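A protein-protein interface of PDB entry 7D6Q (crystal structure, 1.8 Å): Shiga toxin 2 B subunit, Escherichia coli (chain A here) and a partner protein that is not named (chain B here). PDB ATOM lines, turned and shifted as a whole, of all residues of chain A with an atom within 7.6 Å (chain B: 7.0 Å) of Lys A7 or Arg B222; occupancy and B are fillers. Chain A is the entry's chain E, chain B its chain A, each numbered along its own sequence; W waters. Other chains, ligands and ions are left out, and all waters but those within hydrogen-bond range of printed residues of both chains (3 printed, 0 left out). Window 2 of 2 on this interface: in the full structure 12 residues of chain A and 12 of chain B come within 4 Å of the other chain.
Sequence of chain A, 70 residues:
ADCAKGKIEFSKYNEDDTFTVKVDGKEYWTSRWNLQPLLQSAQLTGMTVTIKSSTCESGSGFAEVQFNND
Thr B280 touches Leu A44 (O to CD1, 3.9 Å). Thr A45 touches Arg B222 (C to CA, 3.7 Å). CG of Arg B222 touches N of Gly A46 (3.6 Å).
Of the 12 printed residues of chain B, 4 touch a printed residue of chain A. Among the printed residues, no Asp or Glu carboxylate lies within 4 Å of a Lys or Arg side-chain nitrogen of the other chain.
The side-chain carboxylate (OD2) of Asp B197 is in salt-bridge range of the guanidinium group (NE) of Arg B222 (2.8 Å). NH2 of Arg B204 lies within hydrogen-bond range of OG1 of Thr B280 (3.3 Å). The guanidinium group (NH1) of Arg B219 is in hydrogen-bond range of the backbone carbonyl oxygen (O) of Gly B221 (2.9 Å). NH1 of Arg B219 sits at hydrogen-bond distance from O of Ile B223 (3.0 Å). N of Gly B221 sits at hydrogen-bond distance from OG1 of Thr B280 (2.9 Å). OG1 of Thr A45 lies within hydrogen-bond range of O of Ser A41 (2.8 Å).
NH2 of Arg B219 sits at hydrogen-bond distance from O of Thr A45, 2.6 Å away. The backbone carbonyl oxygen (O) of Arg B222 sits at hydrogen-bond distance from the side-chain amino group (NZ) of Lys A7 (3.0 Å). NH1 of Arg B222 is in hydrogen-bond range of O of Ile A8. NH1 of Arg B222 sits at hydrogen-bond distance from O of Gln A43 (3.0 Å). N of Arg B222 lies within hydrogen-bond range of O of Leu A44 (3.4 Å). The backbone carbonyl oxygen (O) of Gly B221 lies close to the backbone carbonyl oxygen (O) of Leu A44, 3.5 Å away. The backbone carbonyl oxygen (O) of Gly B221 lies close to the backbone carbonyl oxygen (O) of Thr A45, at 3.3 Å.
Water W3 bridges the side-chain carboxylate (OD2) of Asp B197 and the side-chain amino group (NZ) of Lys A7. Water W1 bridges the backbone carbonyl oxygen (O) of Leu A44 (2.8 Å) and the guanidinium group (NH2) of Arg B204 (3.0 Å). Water W2 lies within hydrogen-bond range of the guanidinium group (NH2) of Arg B219 (3.0 Å), the backbone carbonyl oxygen (O) of Asn A69 (3.0 Å) and the backbone carbonyl oxygen (O) of Thr A45 (3.1 Å).
Lys A7 touches just one residue of chain B: Arg B222. Asp A24 touches none of the printed residues of chain B. Printed residues of chain B within 4 Å of Gln A43: Arg B222. Printed residues of chain B within 4 Å of Thr A45: Arg B219 (2.6 Å), Gly B221 (3.3 Å) and Arg B222 (3.7 Å). Asp B197 touches none of the printed residues of chain A. Of chain A, only Leu A44 (3.1 Å) and Thr A45 (3.3 Å) come within 4 Å of Gly B221. Arg B222 touches just these residues of chain A: Lys A7, Ile A8, Gln A43, Leu A44, Thr A45 and Gly A46. The nearest residue of chain A that does not touch Arg B222 is Glu A9 (4.9 Å). The nearest printed residue of chain B that does not touch Thr A45 is Thr B280 (4.1 Å).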
ATOM      1  N   LYS A   5      11.471  10.628 -20.938  1.00  0.00           N
ATOM      2  CA  LYS A   5      12.022   9.691 -19.967  1.00  0.00           C
ATOM      3  C   LYS A   5      13.288  10.275 -19.368  1.00  0.00           C
ATOM      4  O   LYS A   5      14.187  10.700 -20.100  1.00  0.00           O
ATOM      5  CB  LYS A   5      12.323   8.333 -20.610  1.00  0.00           C
ATOM      6  CG  LYS A   5      12.870   7.307 -19.651  1.00  0.00           C
ATOM      7  CD  LYS A   5      12.844   5.922 -20.300  1.00  0.00           C
ATOM      8  CE  LYS A   5      13.562   4.889 -19.460  1.00  0.00           C
ATOM      9  NZ  LYS A   5      14.358   3.974 -20.339  1.00  0.00           N
ATOM     10  N   GLY A   6      13.358  10.301 -18.047  1.00  0.00           N
ATOM     11  CA  GLY A   6      14.526  10.848 -17.386  1.00  0.00           C
ATOM     12  C   GLY A   6      14.210  11.194 -15.949  1.00  0.00           C
ATOM     13  O   GLY A   6      13.117  10.934 -15.450  1.00  0.00           O
ATOM     14  N   LYS A   7      15.206  11.781 -15.287  1.00  0.00           N
ATOM     15  CA  LYS A   7      14.963  12.308 -13.953  1.00  0.00           C
ATOM     16  C   LYS A   7      14.226  13.644 -14.051  1.00  0.00           C
ATOM     17  O   LYS A   7      14.233  14.318 -15.086  1.00  0.00           O
ATOM     18  CB  LYS A   7      16.272  12.479 -13.179  1.00  0.00           C
ATOM     19  CG  LYS A   7      17.034  11.176 -12.923  1.00  0.00           C
ATOM     20  CD  LYS A   7      18.276  11.437 -12.078  1.00  0.00           C
ATOM     21  CE  LYS A   7      19.019  10.146 -11.710  1.00  0.00           C
ATOM     22  NZ  LYS A   7      19.855  10.373 -10.477  1.00  0.00           N
ATOM     23  N   ILE A   8      13.561  14.019 -12.965  1.00  0.00           N
ATOM     24  CA  ILE A   8      12.800  15.266 -12.957  1.00  0.00           C
ATOM     25  C   ILE A   8      13.757  16.424 -12.712  1.00  0.00           C
ATOM     26  O   ILE A   8      14.452  16.464 -11.692  1.00  0.00           O
ATOM     27  CB  ILE A   8      11.687  15.229 -11.902  1.00  0.00           C
ATOM     28  CG1 ILE A   8      10.589  14.256 -12.344  1.00  0.00           C
ATOM     29  CG2 ILE A   8      11.107  16.618 -11.703  1.00  0.00           C
ATOM     30  CD1 ILE A   8       9.632  13.869 -11.206  1.00  0.00           C
ATOM     31  N   GLU A   9      13.803  17.366 -13.654  1.00  0.00           N
ATOM     32  CA  GLU A   9      14.734  18.485 -13.534  1.00  0.00           C
ATOM     33  C   GLU A   9      14.214  19.549 -12.580  1.00  0.00           C
ATOM     34  O   GLU A   9      14.987  20.121 -11.802  1.00  0.00           O
ATOM     35  CB  GLU A   9      15.007  19.104 -14.900  1.00  0.00           C
ATOM     36  CG  GLU A   9      15.977  20.269 -14.803  1.00  0.00           C
ATOM     37  CD  GLU A   9      16.229  20.948 -16.133  1.00  0.00           C
ATOM     38  OE1 GLU A   9      16.814  22.058 -16.123  1.00  0.00           O
ATOM     39  OE2 GLU A   9      15.840  20.375 -17.178  1.00  0.00           O
ATOM     40  N   PHE A  10      12.922  19.856 -12.659  1.00  0.00           N
ATOM     41  CA  PHE A  10      12.271  20.677 -11.648  1.00  0.00           C
ATOM     42  C   PHE A  10      10.792  20.337 -11.663  1.00  0.00           C
ATOM     43  O   PHE A  10      10.285  19.729 -12.613  1.00  0.00           O
ATOM     44  CB  PHE A  10      12.520  22.191 -11.855  1.00  0.00           C
ATOM     45  CG  PHE A  10      11.758  22.819 -13.014  1.00  0.00           C
ATOM     46  CD1 PHE A  10      10.420  23.169 -12.890  1.00  0.00           C
ATOM     47  CD2 PHE A  10      12.407  23.114 -14.201  1.00  0.00           C
ATOM     48  CE1 PHE A  10       9.732  23.747 -13.942  1.00  0.00           C
ATOM     49  CE2 PHE A  10      11.730  23.704 -15.255  1.00  0.00           C
ATOM     50  CZ  PHE A  10      10.386  24.018 -15.125  1.00  0.00           C
ATOM     51  N   VAL A  21       6.175  19.385 -14.453  1.00  0.00           N
ATOM     52  CA  VAL A  21       7.491  18.785 -14.282  1.00  0.00           C
ATOM     53  C   VAL A  21       8.249  18.945 -15.588  1.00  0.00           C
ATOM     54  O   VAL A  21       7.654  18.989 -16.667  1.00  0.00           O
ATOM     55  CB  VAL A  21       7.415  17.299 -13.884  1.00  0.00           C
ATOM     56  CG1 VAL A  21       6.893  17.169 -12.445  1.00  0.00           C
ATOM     57  CG2 VAL A  21       6.503  16.550 -14.865  1.00  0.00           C
ATOM     58  N   LYS A  22       9.570  19.042 -15.484  1.00  0.00           N
ATOM     59  CA  LYS A  22      10.444  19.054 -16.647  1.00  0.00           C
ATOM     60  C   LYS A  22      11.242  17.760 -16.659  1.00  0.00           C
ATOM     61  O   LYS A  22      11.902  17.423 -15.671  1.00  0.00           O
ATOM     62  CB  LYS A  22      11.384  20.260 -16.629  1.00  0.00           C
ATOM     63  CG  LYS A  22      12.122  20.450 -17.943  1.00  0.00           C
ATOM     64  CD  LYS A  22      12.869  21.786 -17.984  1.00  0.00           C
ATOM     65  CE  LYS A  22      13.832  21.852 -19.182  1.00  0.00           C
ATOM     66  NZ  LYS A  22      14.380  23.224 -19.398  1.00  0.00           N
ATOM     67  N   VAL A  23      11.176  17.038 -17.777  1.00  0.00           N
ATOM     68  CA  VAL A  23      11.835  15.744 -17.933  1.00  0.00           C
ATOM     69  C   VAL A  23      12.490  15.738 -19.308  1.00  0.00           C
ATOM     70  O   VAL A  23      11.812  15.974 -20.308  1.00  0.00           O
ATOM     71  CB  VAL A  23      10.849  14.566 -17.811  1.00  0.00           C
ATOM     72  CG1 VAL A  23      11.580  13.215 -17.975  1.00  0.00           C
ATOM     73  CG2 VAL A  23      10.099  14.623 -16.468  1.00  0.00           C
ATOM     74  N   ASP A  24      13.801  15.499 -19.356  1.00  0.00           N
ATOM     75  CA  ASP A  24      14.531  15.402 -20.629  1.00  0.00           C
ATOM     76  C   ASP A  24      14.282  16.623 -21.513  1.00  0.00           C
ATOM     77  O   ASP A  24      13.973  16.513 -22.705  1.00  0.00           O
ATOM     78  CB  ASP A  24      14.166  14.114 -21.372  1.00  0.00           C
ATOM     79  CG  ASP A  24      15.151  13.788 -22.486  1.00  0.00           C
ATOM     80  OD1 ASP A  24      16.334  14.145 -22.346  1.00  0.00           O
ATOM     81  OD2 ASP A  24      14.733  13.193 -23.498  1.00  0.00           O
ATOM     82  N   GLY A  25      14.397  17.802 -20.913  1.00  0.00           N
ATOM     83  CA  GLY A  25      14.253  19.054 -21.628  1.00  0.00           C
ATOM     84  C   GLY A  25      12.839  19.469 -21.991  1.00  0.00           C
ATOM     85  O   GLY A  25      12.672  20.509 -22.646  1.00  0.00           O
ATOM     86  N   GLN A  40       7.037  14.501  -6.792  1.00  0.00           N
ATOM     87  CA  GLN A  40       8.074  15.153  -5.995  1.00  0.00           C
ATOM     88  C   GLN A  40       8.998  14.135  -5.338  1.00  0.00           C
ATOM     89  O   GLN A  40      10.222  14.316  -5.335  1.00  0.00           O
ATOM     90  CB  GLN A  40       7.470  16.073  -4.937  1.00  0.00           C
ATOM     91  CG  GLN A  40       8.585  16.963  -4.350  1.00  0.00           C
ATOM     92  CD  GLN A  40       8.269  17.501  -2.977  1.00  0.00           C
ATOM     93  OE1 GLN A  40       7.792  16.772  -2.097  1.00  0.00           O
ATOM     94  NE2 GLN A  40       8.552  18.788  -2.775  1.00  0.00           N
ATOM     95  N   SER A  41       8.438  13.055  -4.781  1.00  0.00           N
ATOM     96  CA  SER A  41       9.284  11.990  -4.260  1.00  0.00           C
ATOM     97  C   SER A  41      10.215  11.475  -5.348  1.00  0.00           C
ATOM     98  O   SER A  41      11.427  11.334  -5.128  1.00  0.00           O
ATOM     99  CB  SER A  41       8.426  10.859  -3.693  1.00  0.00           C
ATOM    100  OG  SER A  41       7.767  11.298  -2.515  1.00  0.00           O
ATOM    101  N   ALA A  42       9.668  11.255  -6.547  1.00  0.00           N
ATOM    102  CA  ALA A  42      10.508  10.793  -7.646  1.00  0.00           C
ATOM    103  C   ALA A  42      11.620  11.793  -7.920  1.00  0.00           C
ATOM    104  O   ALA A  42      12.766  11.406  -8.172  1.00  0.00           O
ATOM    105  CB  ALA A  42       9.661  10.567  -8.903  1.00  0.00           C
ATOM    106  N   GLN A  43      11.304  13.091  -7.836  1.00  0.00           N
ATOM    107  CA  GLN A  43      12.318  14.108  -8.078  1.00  0.00           C
ATOM    108  C   GLN A  43      13.399  14.075  -7.006  1.00  0.00           C
ATOM    109  O   GLN A  43      14.596  14.133  -7.320  1.00  0.00           O
ATOM    110  CB  GLN A  43      11.664  15.497  -8.145  1.00  0.00           C
ATOM    111  CG  GLN A  43      12.678  16.647  -8.229  1.00  0.00           C
ATOM    112  CD  GLN A  43      11.999  18.011  -8.201  1.00  0.00           C
ATOM    113  OE1 GLN A  43      10.774  18.095  -8.070  1.00  0.00           O
ATOM    114  NE2 GLN A  43      12.787  19.082  -8.340  1.00  0.00           N
ATOM    115  N   LEU A  44      13.011  13.960  -5.732  1.00  0.00           N
ATOM    116  CA  LEU A  44      14.029  14.133  -4.711  1.00  0.00           C
ATOM    117  C   LEU A  44      14.859  12.875  -4.501  1.00  0.00           C
ATOM    118  O   LEU A  44      15.941  12.956  -3.916  1.00  0.00           O
ATOM    119  CB  LEU A  44      13.391  14.590  -3.400  1.00  0.00           C
ATOM    120  CG  LEU A  44      12.462  13.646  -2.644  1.00  0.00           C
ATOM    121  CD1 LEU A  44      13.247  12.865  -1.601  1.00  0.00           C
ATOM    122  CD2 LEU A  44      11.380  14.488  -1.975  1.00  0.00           C
ATOM    123  N   THR A  45      14.392  11.728  -4.988  1.00  0.00           N
ATOM    124  CA  THR A  45      15.131  10.476  -4.889  1.00  0.00           C
ATOM    125  C   THR A  45      15.832  10.093  -6.185  1.00  0.00           C
ATOM    126  O   THR A  45      16.504   9.055  -6.219  1.00  0.00           O
ATOM    127  CB  THR A  45      14.199   9.332  -4.478  1.00  0.00           C
ATOM    128  OG1 THR A  45      13.181   9.157  -5.479  1.00  0.00           O
ATOM    129  CG2 THR A  45      13.556   9.623  -3.113  1.00  0.00           C
ATOM    130  N   GLY A  46      15.669  10.872  -7.252  1.00  0.00           N
ATOM    131  CA  GLY A  46      16.338  10.553  -8.501  1.00  0.00           C
ATOM    132  C   GLY A  46      15.765   9.376  -9.257  1.00  0.00           C
ATOM    133  O   GLY A  46      16.500   8.698  -9.987  1.00  0.00           O
ATOM    134  N   MET A  47      14.471   9.111  -9.116  1.00  0.00           N
ATOM    135  CA  MET A  47      13.843   8.089  -9.941  1.00  0.00           C
ATOM    136  C   MET A  47      13.820   8.505 -11.407  1.00  0.00           C
ATOM    137  O   MET A  47      13.749   9.688 -11.743  1.00  0.00           O
ATOM    138  CB  MET A  47      12.406   7.819  -9.484  1.00  0.00           C
ATOM    139  CG  MET A  47      12.257   7.220  -8.086  1.00  0.00           C
ATOM    140  SD  MET A  47      10.516   6.820  -7.739  1.00  0.00           S
ATOM    141  CE  MET A  47      10.533   5.049  -8.005  1.00  0.00           C
ATOM    142  N   THR A  48      13.868   7.510 -12.287  1.00  0.00           N
ATOM    143  CA  THR A  48      13.604   7.727 -13.705  1.00  0.00           C
ATOM    144  C   THR A  48      12.098   7.675 -13.935  1.00  0.00           C
ATOM    145  O   THR A  48      11.451   6.666 -13.621  1.00  0.00           O
ATOM    146  CB  THR A  48      14.306   6.662 -14.555  1.00  0.00           C
ATOM    147  OG1 THR A  48      15.719   6.854 -14.485  1.00  0.00           O
ATOM    148  CG2 THR A  48      13.852   6.754 -16.016  1.00  0.00           C
ATOM    149  N   VAL A  49      11.528   8.746 -14.470  1.00  0.00           N
ATOM    150  CA  VAL A  49      10.095   8.754 -14.764  1.00  0.00           C
ATOM    151  C   VAL A  49       9.906   8.701 -16.273  1.00  0.00           C
ATOM    152  O   VAL A  49      10.724   9.217 -17.038  1.00  0.00           O
ATOM    153  CB  VAL A  49       9.353   9.969 -14.155  1.00  0.00           C
ATOM    154  CG1 VAL A  49       9.659  10.105 -12.654  1.00  0.00           C
ATOM    155  CG2 VAL A  49       9.671  11.261 -14.901  1.00  0.00           C
ATOM    156  N   THR A  50       8.825   8.045 -16.704  1.00  0.00           N
ATOM    157  CA  THR A  50       8.412   8.039 -18.108  1.00  0.00           C
ATOM    158  C   THR A  50       7.035   8.681 -18.192  1.00  0.00           C
ATOM    159  O   THR A  50       6.044   8.088 -17.750  1.00  0.00           O
ATOM    160  CB  THR A  50       8.376   6.625 -18.692  1.00  0.00           C
ATOM    161  OG1 THR A  50       9.640   5.986 -18.500  1.00  0.00           O
ATOM    162  CG2 THR A  50       8.071   6.688 -20.186  1.00  0.00           C
ATOM    163  N   ASN A  68      10.634   4.312 -12.133  1.00  0.00           N
ATOM    164  CA  ASN A  68      11.685   3.306 -12.024  1.00  0.00           C
ATOM    165  C   ASN A  68      12.795   3.824 -11.123  1.00  0.00           C
ATOM    166  O   ASN A  68      13.149   5.005 -11.187  1.00  0.00           O
ATOM    167  CB  ASN A  68      12.301   2.975 -13.402  1.00  0.00           C
ATOM    168  CG  ASN A  68      11.426   2.078 -14.236  1.00  0.00           C
ATOM    169  OD1 ASN A  68      10.534   2.542 -14.940  1.00  0.00           O
ATOM    170  ND2 ASN A  68      11.688   0.781 -14.176  1.00  0.00           N
ATOM    171  N   ASN A  69      13.382   2.931 -10.318  1.00  0.00           N
ATOM    172  CA  ASN A  69      14.503   3.349  -9.479  1.00  0.00           C
ATOM    173  C   ASN A  69      15.714   3.728 -10.322  1.00  0.00           C
ATOM    174  O   ASN A  69      16.440   4.669  -9.981  1.00  0.00           O
ATOM    175  CB  ASN A  69      14.868   2.251  -8.486  1.00  0.00           C
ATOM    176  CG  ASN A  69      13.970   2.254  -7.271  1.00  0.00           C
ATOM    177  OD1 ASN A  69      13.335   3.261  -6.962  1.00  0.00           O
ATOM    178  ND2 ASN A  69      13.910   1.126  -6.576  1.00  0.00           N
ATOM    179  N   ASP A  70      15.948   3.024 -11.423  1.00  0.00           N
ATOM    180  CA  ASP A  70      17.088   3.383 -12.275  1.00  0.00           C
ATOM    181  C   ASP A  70      16.826   3.124 -13.756  1.00  0.00           C
ATOM    182  O   ASP A  70      16.104   3.881 -14.407  1.00  0.00           O
ATOM    183  CB  ASP A  70      18.350   2.633 -11.826  1.00  0.00           C
ATOM    184  CG  ASP A  70      18.133   1.131 -11.709  1.00  0.00           C
ATOM    185  OD1 ASP A  70      17.596   0.518 -12.658  1.00  0.00           O
ATOM    186  OD2 ASP A  70      18.499   0.563 -10.657  1.00  0.00           O
ATOM    187  N   PRO B 193      24.122  15.963 -16.666  1.00  0.00           N
ATOM    188  CA  PRO B 193      23.247  16.207 -15.509  1.00  0.00           C
ATOM    189  C   PRO B 193      23.698  15.456 -14.272  1.00  0.00           C
ATOM    190  O   PRO B 193      23.593  15.993 -13.163  1.00  0.00           O
ATOM    191  CB  PRO B 193      21.876  15.734 -16.014  1.00  0.00           C
ATOM    192  CG  PRO B 193      21.939  15.978 -17.482  1.00  0.00           C
ATOM    193  CD  PRO B 193      23.351  15.640 -17.882  1.00  0.00           C
ATOM    194  N   GLY B 194      24.211  14.233 -14.432  1.00  0.00           N
ATOM    195  CA  GLY B 194      24.700  13.487 -13.279  1.00  0.00           C
ATOM    196  C   GLY B 194      25.915  14.126 -12.633  1.00  0.00           C
ATOM    197  O   GLY B 194      26.021  14.169 -11.399  1.00  0.00           O
ATOM    198  N   ASP B 197      24.546  17.085 -10.647  1.00  0.00           N
ATOM    199  CA  ASP B 197      23.911  16.625  -9.413  1.00  0.00           C
ATOM    200  C   ASP B 197      24.935  16.240  -8.350  1.00  0.00           C
ATOM    201  O   ASP B 197      24.736  16.511  -7.155  1.00  0.00           O
ATOM    202  CB  ASP B 197      22.994  15.435  -9.706  1.00  0.00           C
ATOM    203  CG  ASP B 197      21.556  15.856  -9.955  1.00  0.00           C
ATOM    204  OD1 ASP B 197      21.236  17.037  -9.717  1.00  0.00           O
ATOM    205  OD2 ASP B 197      20.754  15.010 -10.404  1.00  0.00           O
ATOM    206  N   ASN B 201      25.240  17.957  -4.535  1.00  0.00           N
ATOM    207  CA  ASN B 201      24.989  17.155  -3.341  1.00  0.00           C
ATOM    208  C   ASN B 201      26.247  16.855  -2.539  1.00  0.00           C
ATOM    209  O   ASN B 201      26.237  15.926  -1.724  1.00  0.00           O
ATOM    210  CB  ASN B 201      24.314  15.842  -3.733  1.00  0.00           C
ATOM    211  CG  ASN B 201      22.880  16.044  -4.151  1.00  0.00           C
ATOM    212  OD1 ASN B 201      21.980  16.043  -3.315  1.00  0.00           O
ATOM    213  ND2 ASN B 201      22.661  16.236  -5.446  1.00  0.00           N
ATOM    214  N   ARG B 204      25.780  16.899   1.328  1.00  0.00           N
ATOM    215  CA  ARG B 204      24.960  15.792   1.814  1.00  0.00           C
ATOM    216  C   ARG B 204      25.717  14.472   1.733  1.00  0.00           C
ATOM    217  O   ARG B 204      25.689  13.652   2.676  1.00  0.00           O
ATOM    218  CB  ARG B 204      23.658  15.731   1.018  1.00  0.00           C
ATOM    219  CG  ARG B 204      22.800  16.991   1.188  1.00  0.00           C
ATOM    220  CD  ARG B 204      21.690  17.040   0.158  1.00  0.00           C
ATOM    221  NE  ARG B 204      20.621  16.076   0.432  1.00  0.00           N
ATOM    222  CZ  ARG B 204      19.598  15.865  -0.391  1.00  0.00           C
ATOM    223  NH1 ARG B 204      19.521  16.550  -1.528  1.00  0.00           N
ATOM    224  NH2 ARG B 204      18.654  14.980  -0.084  1.00  0.00           N
ATOM    225  N   ARG B 219      22.185   5.820  -0.457  1.00  0.00           N
ATOM    226  CA  ARG B 219      21.221   6.684  -1.124  1.00  0.00           C
ATOM    227  C   ARG B 219      21.268   8.040  -0.443  1.00  0.00           C
ATOM    228  O   ARG B 219      21.126   8.126   0.781  1.00  0.00           O
ATOM    229  CB  ARG B 219      19.808   6.087  -1.082  1.00  0.00           C
ATOM    230  CG  ARG B 219      19.659   4.775  -1.861  1.00  0.00           C
ATOM    231  CD  ARG B 219      19.615   5.010  -3.372  1.00  0.00           C
ATOM    232  NE  ARG B 219      18.302   5.472  -3.812  1.00  0.00           N
ATOM    233  CZ  ARG B 219      18.034   6.710  -4.217  1.00  0.00           C
ATOM    234  NH1 ARG B 219      18.988   7.641  -4.262  1.00  0.00           N
ATOM    235  NH2 ARG B 219      16.798   7.018  -4.583  1.00  0.00           N
ATOM    236  N   VAL B 220      21.534   9.083  -1.224  1.00  0.00           N
ATOM    237  CA  VAL B 220      21.584  10.448  -0.720  1.00  0.00           C
ATOM    238  C   VAL B 220      20.842  11.298  -1.731  1.00  0.00           C
ATOM    239  O   VAL B 220      21.382  11.609  -2.794  1.00  0.00           O
ATOM    240  CB  VAL B 220      23.030  10.952  -0.545  1.00  0.00           C
ATOM    241  CG1 VAL B 220      23.012  12.398  -0.056  1.00  0.00           C
ATOM    242  CG2 VAL B 220      23.799  10.073   0.431  1.00  0.00           C
ATOM    243  N   GLY B 221      19.601  11.667  -1.418  1.00  0.00           N
ATOM    244  CA  GLY B 221      18.770  12.352  -2.395  1.00  0.00           C
ATOM    245  C   GLY B 221      18.712  11.635  -3.731  1.00  0.00           C
ATOM    246  O   GLY B 221      18.331  10.460  -3.807  1.00  0.00           O
ATOM    247  N   ARG B 222      19.126  12.329  -4.793  1.00  0.00           N
ATOM    248  CA  ARG B 222      19.118  11.785  -6.147  1.00  0.00           C
ATOM    249  C   ARG B 222      20.315  10.890  -6.455  1.00  0.00           C
ATOM    250  O   ARG B 222      20.365  10.319  -7.548  1.00  0.00           O
ATOM    251  CB  ARG B 222      19.073  12.939  -7.158  1.00  0.00           C
ATOM    252  CG  ARG B 222      17.802  13.798  -7.051  1.00  0.00           C
ATOM    253  CD  ARG B 222      17.961  15.159  -7.709  1.00  0.00           C
ATOM    254  NE  ARG B 222      18.217  15.142  -9.158  1.00  0.00           N
ATOM    255  CZ  ARG B 222      17.276  15.094 -10.101  1.00  0.00           C
ATOM    256  NH1 ARG B 222      15.985  15.004  -9.774  1.00  0.00           N
ATOM    257  NH2 ARG B 222      17.625  15.132 -11.385  1.00  0.00           N
ATOM    258  N   ILE B 223      21.248  10.744  -5.519  1.00  0.00           N
ATOM    259  CA  ILE B 223      22.512  10.037  -5.722  1.00  0.00           C
ATOM    260  C   ILE B 223      22.366   8.622  -5.182  1.00  0.00           C
ATOM    261  O   ILE B 223      21.859   8.422  -4.069  1.00  0.00           O
ATOM    262  CB  ILE B 223      23.669  10.767  -5.012  1.00  0.00           C
ATOM    263  CG1 ILE B 223      23.711  12.259  -5.364  1.00  0.00           C
ATOM    264  CG2 ILE B 223      25.018  10.084  -5.305  1.00  0.00           C
ATOM    265  CD1 ILE B 223      23.765  12.552  -6.858  1.00  0.00           C
ATOM    266  N   SER B 224      22.819   7.635  -5.959  1.00  0.00           N
ATOM    267  CA  SER B 224      22.796   6.247  -5.525  1.00  0.00           C
ATOM    268  C   SER B 224      24.124   5.583  -5.845  1.00  0.00           C
ATOM    269  O   SER B 224      24.665   5.764  -6.938  1.00  0.00           O
ATOM    270  CB  SER B 224      21.656   5.458  -6.193  1.00  0.00           C
ATOM    271  OG  SER B 224      21.533   5.770  -7.570  1.00  0.00           O
ATOM    272  N   THR B 280      16.334  12.268   3.296  1.00  0.00           N
ATOM    273  CA  THR B 280      15.697  11.794   2.068  1.00  0.00           C
ATOM    274  C   THR B 280      14.501  10.895   2.390  1.00  0.00           C
ATOM    275  O   THR B 280      13.386  11.076   1.854  1.00  0.00           O
ATOM    276  CB  THR B 280      16.723  11.041   1.211  1.00  0.00           C
ATOM    277  OG1 THR B 280      17.807  11.922   0.862  1.00  0.00           O
ATOM    278  CG2 THR B 280      16.080  10.503  -0.052  1.00  0.00           C
HETATM  279  O   HOH W   1      16.830  15.189  -2.489  1.00  0.00           O
HETATM  280  O   HOH W   2      16.227   6.225  -7.391  1.00  0.00           O
HETATM  281  O   HOH W   3      21.565  12.585 -10.720  1.00  0.00           O
